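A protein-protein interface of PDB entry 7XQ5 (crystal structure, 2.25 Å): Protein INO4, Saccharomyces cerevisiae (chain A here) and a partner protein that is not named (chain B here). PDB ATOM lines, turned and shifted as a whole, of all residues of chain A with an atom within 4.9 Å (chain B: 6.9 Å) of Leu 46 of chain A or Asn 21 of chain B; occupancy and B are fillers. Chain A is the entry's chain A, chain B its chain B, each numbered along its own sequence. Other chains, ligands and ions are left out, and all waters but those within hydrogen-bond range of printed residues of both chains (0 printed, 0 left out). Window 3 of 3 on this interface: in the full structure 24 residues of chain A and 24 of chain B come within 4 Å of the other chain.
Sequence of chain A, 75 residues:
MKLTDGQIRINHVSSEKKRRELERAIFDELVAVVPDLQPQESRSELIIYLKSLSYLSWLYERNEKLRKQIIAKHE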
ATOM      1  N   SER A  44     -12.506  25.968 -16.959  1.00  0.00           N
ATOM      2  CA  SER A  44     -11.060  26.123 -16.769  1.00  0.00           C
ATOM      3  C   SER A  44     -10.834  26.463 -15.307  1.00  0.00           C
ATOM      4  O   SER A  44     -10.897  27.634 -14.913  1.00  0.00           O
ATOM      5  CB  SER A  44     -10.514  27.225 -17.655  1.00  0.00           C
ATOM      6  OG  SER A  44     -10.986  27.046 -18.982  1.00  0.00           O
ATOM      7  N   GLU A  45     -10.584  25.432 -14.491  1.00  0.00           N
ATOM      8  CA  GLU A  45     -10.528  25.637 -13.045  1.00  0.00           C
ATOM      9  C   GLU A  45      -9.480  26.679 -12.684  1.00  0.00           C
ATOM     10  O   GLU A  45      -9.751  27.586 -11.890  1.00  0.00           O
ATOM     11  CB  GLU A  45     -10.245  24.325 -12.321  1.00  0.00           C
ATOM     12  CG  GLU A  45     -11.397  23.378 -12.280  1.00  0.00           C
ATOM     13  CD  GLU A  45     -11.162  22.248 -11.308  1.00  0.00           C
ATOM     14  OE1 GLU A  45     -11.005  22.517 -10.089  1.00  0.00           O
ATOM     15  OE2 GLU A  45     -11.118  21.092 -11.765  1.00  0.00           O
ATOM     16  N   LEU A  46      -8.278  26.569 -13.262  1.00  0.00           N
ATOM     17  CA  LEU A  46      -7.199  27.489 -12.905  1.00  0.00           C
ATOM     18  C   LEU A  46      -7.657  28.929 -13.060  1.00  0.00           C
ATOM     19  O   LEU A  46      -7.468  29.755 -12.164  1.00  0.00           O
ATOM     20  CB  LEU A  46      -5.958  27.236 -13.765  1.00  0.00           C
ATOM     21  CG  LEU A  46      -4.810  28.248 -13.598  1.00  0.00           C
ATOM     22  CD1 LEU A  46      -4.022  27.944 -12.373  1.00  0.00           C
ATOM     23  CD2 LEU A  46      -3.879  28.217 -14.787  1.00  0.00           C
ATOM     24  N   ILE A  47      -8.317  29.231 -14.172  1.00  0.00           N
ATOM     25  CA  ILE A  47      -8.708  30.609 -14.448  1.00  0.00           C
ATOM     26  C   ILE A  47      -9.833  31.037 -13.521  1.00  0.00           C
ATOM     27  O   ILE A  47      -9.867  32.177 -13.043  1.00  0.00           O
ATOM     28  CB  ILE A  47      -9.111  30.756 -15.925  1.00  0.00           C
ATOM     29  CG1 ILE A  47      -7.894  30.536 -16.824  1.00  0.00           C
ATOM     30  CG2 ILE A  47      -9.720  32.113 -16.178  1.00  0.00           C
ATOM     31  CD1 ILE A  47      -8.232  30.535 -18.292  1.00  0.00           C
ATOM     32  N   ILE A  48     -10.776  30.134 -13.258  1.00  0.00           N
ATOM     33  CA  ILE A  48     -11.858  30.445 -12.329  1.00  0.00           C
ATOM     34  C   ILE A  48     -11.293  30.845 -10.980  1.00  0.00           C
ATOM     35  O   ILE A  48     -11.680  31.864 -10.402  1.00  0.00           O
ATOM     36  CB  ILE A  48     -12.812  29.249 -12.203  1.00  0.00           C
ATOM     37  CG1 ILE A  48     -13.519  29.012 -13.545  1.00  0.00           C
ATOM     38  CG2 ILE A  48     -13.815  29.500 -11.088  1.00  0.00           C
ATOM     39  CD1 ILE A  48     -14.102  27.615 -13.702  1.00  0.00           C
ATOM     40  N   TYR A  49     -10.341  30.068 -10.470  1.00  0.00           N
ATOM     41  CA  TYR A  49      -9.815  30.350  -9.139  1.00  0.00           C
ATOM     42  C   TYR A  49      -9.052  31.663  -9.124  1.00  0.00           C
ATOM     43  O   TYR A  49      -9.244  32.483  -8.226  1.00  0.00           O
ATOM     44  CB  TYR A  49      -8.937  29.183  -8.658  1.00  0.00           C
ATOM     45  CG  TYR A  49      -9.679  27.853  -8.627  1.00  0.00           C
ATOM     46  CD1 TYR A  49     -11.066  27.822  -8.539  1.00  0.00           C
ATOM     47  CD2 TYR A  49      -9.003  26.641  -8.677  1.00  0.00           C
ATOM     48  CE1 TYR A  49     -11.764  26.634  -8.514  1.00  0.00           C
ATOM     49  CE2 TYR A  49      -9.699  25.441  -8.647  1.00  0.00           C
ATOM     50  CZ  TYR A  49     -11.088  25.452  -8.568  1.00  0.00           C
ATOM     51  OH  TYR A  49     -11.822  24.280  -8.542  1.00  0.00           O
ATOM     52  N   LEU A  50      -8.218  31.903 -10.133  1.00  0.00           N
ATOM     53  CA  LEU A  50      -7.437  33.138 -10.164  1.00  0.00           C
ATOM     54  C   LEU A  50      -8.339  34.359 -10.307  1.00  0.00           C
ATOM     55  O   LEU A  50      -8.166  35.356  -9.599  1.00  0.00           O
ATOM     56  CB  LEU A  50      -6.424  33.088 -11.305  1.00  0.00           C
ATOM     57  CG  LEU A  50      -5.271  32.099 -11.137  1.00  0.00           C
ATOM     58  CD1 LEU A  50      -4.383  32.129 -12.351  1.00  0.00           C
ATOM     59  CD2 LEU A  50      -4.473  32.426  -9.892  1.00  0.00           C
ATOM     60  N   LYS B  16      -0.287  16.429 -15.234  1.00  0.00           N
ATOM     61  CA  LYS B  16      -0.008  16.475 -13.810  1.00  0.00           C
ATOM     62  C   LYS B  16       0.458  17.862 -13.388  1.00  0.00           C
ATOM     63  O   LYS B  16       0.104  18.329 -12.301  1.00  0.00           O
ATOM     64  CB  LYS B  16       1.020  15.412 -13.449  1.00  0.00           C
ATOM     65  CG  LYS B  16       1.321  15.382 -11.990  1.00  0.00           C
ATOM     66  CD  LYS B  16       1.915  14.068 -11.523  1.00  0.00           C
ATOM     67  CE  LYS B  16       2.224  14.162 -10.015  1.00  0.00           C
ATOM     68  NZ  LYS B  16       2.897  12.948  -9.473  1.00  0.00           N
ATOM     69  N   ILE B  17       1.189  18.566 -14.253  1.00  0.00           N
ATOM     70  CA  ILE B  17       1.607  19.923 -13.924  1.00  0.00           C
ATOM     71  C   ILE B  17       0.418  20.875 -13.951  1.00  0.00           C
ATOM     72  O   ILE B  17       0.322  21.780 -13.118  1.00  0.00           O
ATOM     73  CB  ILE B  17       2.740  20.372 -14.869  1.00  0.00           C
ATOM     74  CG1 ILE B  17       4.016  19.605 -14.533  1.00  0.00           C
ATOM     75  CG2 ILE B  17       2.998  21.871 -14.772  1.00  0.00           C
ATOM     76  CD1 ILE B  17       5.098  19.791 -15.532  1.00  0.00           C
ATOM     77  N   ARG B  18      -0.497  20.705 -14.908  1.00  0.00           N
ATOM     78  CA  ARG B  18      -1.729  21.490 -14.882  1.00  0.00           C
ATOM     79  C   ARG B  18      -2.494  21.272 -13.573  1.00  0.00           C
ATOM     80  O   ARG B  18      -3.051  22.225 -13.006  1.00  0.00           O
ATOM     81  CB  ARG B  18      -2.617  21.140 -16.079  1.00  0.00           C
ATOM     82  CG  ARG B  18      -2.296  21.874 -17.397  1.00  0.00           C
ATOM     83  CD  ARG B  18      -3.192  21.411 -18.573  1.00  0.00           C
ATOM     84  NE  ARG B  18      -4.584  21.299 -18.144  1.00  0.00           N
ATOM     85  CZ  ARG B  18      -5.444  22.310 -18.112  1.00  0.00           C
ATOM     86  NH1 ARG B  18      -5.112  23.515 -18.549  1.00  0.00           N
ATOM     87  NH2 ARG B  18      -6.672  22.105 -17.632  1.00  0.00           N
ATOM     88  N   ARG B  19      -2.542  20.026 -13.077  1.00  0.00           N
ATOM     89  CA  ARG B  19      -3.228  19.777 -11.809  1.00  0.00           C
ATOM     90  C   ARG B  19      -2.509  20.477 -10.664  1.00  0.00           C
ATOM     91  O   ARG B  19      -3.152  21.068  -9.787  1.00  0.00           O
ATOM     92  CB  ARG B  19      -3.354  18.272 -11.527  1.00  0.00           C
ATOM     93  CG  ARG B  19      -4.339  17.535 -12.497  1.00  0.00           C
ATOM     94  CD  ARG B  19      -4.748  16.110 -12.027  1.00  0.00           C
ATOM     95  NE  ARG B  19      -3.608  15.198 -11.982  1.00  0.00           N
ATOM     96  CZ  ARG B  19      -3.163  14.503 -13.026  1.00  0.00           C
ATOM     97  NH1 ARG B  19      -3.791  14.527 -14.194  1.00  0.00           N
ATOM     98  NH2 ARG B  19      -2.053  13.772 -12.897  1.00  0.00           N
ATOM     99  N   ILE B  20      -1.177  20.441 -10.665  1.00  0.00           N
ATOM    100  CA  ILE B  20      -0.427  21.107  -9.607  1.00  0.00           C
ATOM    101  C   ILE B  20      -0.716  22.599  -9.625  1.00  0.00           C
ATOM    102  O   ILE B  20      -1.104  23.177  -8.605  1.00  0.00           O
ATOM    103  CB  ILE B  20       1.075  20.807  -9.734  1.00  0.00           C
ATOM    104  CG1 ILE B  20       1.320  19.321  -9.531  1.00  0.00           C
ATOM    105  CG2 ILE B  20       1.863  21.547  -8.686  1.00  0.00           C
ATOM    106  CD1 ILE B  20       2.745  18.916  -9.738  1.00  0.00           C
ATOM    107  N   ASN B  21      -0.590  23.240 -10.795  1.00  0.00           N
ATOM    108  CA  ASN B  21      -0.860  24.674 -10.858  1.00  0.00           C
ATOM    109  C   ASN B  21      -2.295  24.994 -10.485  1.00  0.00           C
ATOM    110  O   ASN B  21      -2.560  26.035  -9.875  1.00  0.00           O
ATOM    111  CB  ASN B  21      -0.552  25.233 -12.242  1.00  0.00           C
ATOM    112  CG  ASN B  21       0.904  25.091 -12.600  1.00  0.00           C
ATOM    113  OD1 ASN B  21       1.750  24.869 -11.731  1.00  0.00           O
ATOM    114  ND2 ASN B  21       1.208  25.186 -13.891  1.00  0.00           N
ATOM    115  N   THR B  22      -3.241  24.133 -10.861  1.00  0.00           N
ATOM    116  CA  THR B  22      -4.625  24.383 -10.482  1.00  0.00           C
ATOM    117  C   THR B  22      -4.785  24.319  -8.966  1.00  0.00           C
ATOM    118  O   THR B  22      -5.418  25.189  -8.358  1.00  0.00           O
ATOM    119  CB  THR B  22      -5.542  23.373 -11.168  1.00  0.00           C
ATOM    120  OG1 THR B  22      -5.279  23.377 -12.573  1.00  0.00           O
ATOM    121  CG2 THR B  22      -7.001  23.718 -10.918  1.00  0.00           C
ATOM    122  N   LYS B  23      -4.190  23.302  -8.342  1.00  0.00           N
ATOM    123  CA  LYS B  23      -4.231  23.162  -6.893  1.00  0.00           C
ATOM    124  C   LYS B  23      -3.608  24.373  -6.198  1.00  0.00           C
ATOM    125  O   LYS B  23      -4.169  24.883  -5.220  1.00  0.00           O
ATOM    126  CB  LYS B  23      -3.518  21.866  -6.497  1.00  0.00           C
ATOM    127  CG  LYS B  23      -3.692  21.400  -5.057  1.00  0.00           C
ATOM    128  CD  LYS B  23      -3.754  19.865  -5.011  1.00  0.00           C
ATOM    129  CE  LYS B  23      -2.850  19.298  -3.938  1.00  0.00           C
ATOM    130  NZ  LYS B  23      -3.164  19.899  -2.612  1.00  0.00           N
ATOM    131  N   GLU B  24      -2.465  24.865  -6.698  1.00  0.00           N
ATOM    132  CA  GLU B  24      -1.860  26.060  -6.104  1.00  0.00           C
ATOM    133  C   GLU B  24      -2.788  27.259  -6.204  1.00  0.00           C
ATOM    134  O   GLU B  24      -2.919  28.031  -5.251  1.00  0.00           O
ATOM    135  CB  GLU B  24      -0.529  26.394  -6.771  1.00  0.00           C
ATOM    136  CG  GLU B  24       0.554  25.373  -6.534  1.00  0.00           C
ATOM    137  CD  GLU B  24       1.886  25.766  -7.178  1.00  0.00           C
ATOM    138  OE1 GLU B  24       1.944  26.807  -7.895  1.00  0.00           O
ATOM    139  OE2 GLU B  24       2.872  25.019  -6.961  1.00  0.00           O
ATOM    140  N   ALA B  25      -3.431  27.449  -7.355  1.00  0.00           N
ATOM    141  CA  ALA B  25      -4.359  28.566  -7.468  1.00  0.00           C
ATOM    142  C   ALA B  25      -5.528  28.399  -6.510  1.00  0.00           C
ATOM    143  O   ALA B  25      -6.020  29.378  -5.935  1.00  0.00           O
ATOM    144  CB  ALA B  25      -4.871  28.686  -8.897  1.00  0.00           C
ATOM    145  N   PHE B  26      -5.996  27.166  -6.348  1.00  0.00           N
ATOM    146  CA  PHE B  26      -7.121  26.892  -5.463  1.00  0.00           C
ATOM    147  C   PHE B  26      -6.749  27.172  -4.015  1.00  0.00           C
ATOM    148  O   PHE B  26      -7.513  27.801  -3.273  1.00  0.00           O
ATOM    149  CB  PHE B  26      -7.559  25.443  -5.636  1.00  0.00           C
ATOM    150  CG  PHE B  26      -8.769  25.062  -4.821  1.00  0.00           C
ATOM    151  CD1 PHE B  26      -9.992  25.654  -5.053  1.00  0.00           C
ATOM    152  CD2 PHE B  26      -8.685  24.075  -3.855  1.00  0.00           C
ATOM    153  CE1 PHE B  26     -11.098  25.291  -4.330  1.00  0.00           C
ATOM    154  CE2 PHE B  26      -9.793  23.707  -3.126  1.00  0.00           C
ATOM    155  CZ  PHE B  26     -10.997  24.304  -3.370  1.00  0.00           C
ATOM    156  N   ARG B  28      -4.397  29.203  -2.916  1.00  0.00           N
ATOM    157  CA  ARG B  28      -4.334  30.652  -2.770  1.00  0.00           C
ATOM    158  C   ARG B  28      -5.724  31.238  -2.596  1.00  0.00           C
ATOM    159  O   ARG B  28      -5.960  32.053  -1.704  1.00  0.00           O
ATOM    160  CB  ARG B  28      -3.646  31.272  -3.976  1.00  0.00           C
ATOM    161  CG  ARG B  28      -2.134  31.122  -3.942  1.00  0.00           C
ATOM    162  CD  ARG B  28      -1.488  31.714  -5.198  1.00  0.00           C
ATOM    163  NE  ARG B  28      -0.037  31.685  -5.082  1.00  0.00           N
ATOM    164  CZ  ARG B  28       0.786  31.192  -5.998  1.00  0.00           C
ATOM    165  NH1 ARG B  28       0.335  30.709  -7.150  1.00  0.00           N
ATOM    166  NH2 ARG B  28       2.096  31.201  -5.760  1.00  0.00           N
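OG1 of Thr 22 of chain B lies within hydrogen-bond range of O of Arg 18 of chain B (2.5 Å). OE1 of Glu 45 of chain A sits at hydrogen-bond distance from OH of Tyr 49 of chain A (2.5 Å).
CG2 of Thr 22 of chain B touches CB of Glu 45 of chain A, at 3.6 Å. CD1 of Leu 46 of chain A touches O of Asn 21 of chain B (3.5 Å). Thr 22 of chain B touches Leu 46 of chain A. Leu 46 of chain A touches Ala 25 of chain B. Thr 22 of chain B touches Tyr 49 of chain A (O to CD2, 3.9 Å). Ala 25 of chain B touches Tyr 49 of chain A. CB of Phe 26 of chain B touches CD2 of Tyr 49 of chain A, 3.6 Å away. Leu 50 of chain A touches Ala 25 of chain B (CD2 to CB, 3.9 Å).
Ser 44 of chain A touches none of the printed residues of chain B. Of the printed residues of chain B, Glu 45 of chain A touches Thr 22 (3.6 Å). Printed residues of chain B within 4 Å of Leu 50 of chain A: Ala 25. Of chain A, only Leu 46 (3.5 Å) comes within 4 Å of Asn 21 of chain B. Printed residues of chain A within 4 Å of Thr 22 of chain B: Glu 45 (3.6 Å), Leu 46 (3.9 Å) and Tyr 49 (3.9 Å). Of the printed residues of chain A, Phe 26 of chain B touches Tyr 49 (3.6 Å). The nearest residue of chain B that does not touch Leu 46 of chain A is Arg 18 of chain B (5.8 Å).
Of the 12 printed residues of chain B, 4 touch a printed residue of chain A. Printed residues of chain B that touch a printed residue of chain A: Asn 21, Thr 22, Ala 25 and Phe 26. Of the 7 printed residues of chain A, 4 touch a printed residue of chain B. Printed residues of chain A that touch a printed residue of chain B: Glu 45, Leu 46, Tyr 49 and Leu 50. Hydrophobic or aromatic side chains of chain A within 4 Å of the printed part of chain B: Leu 46, Tyr 49 and Leu 50.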
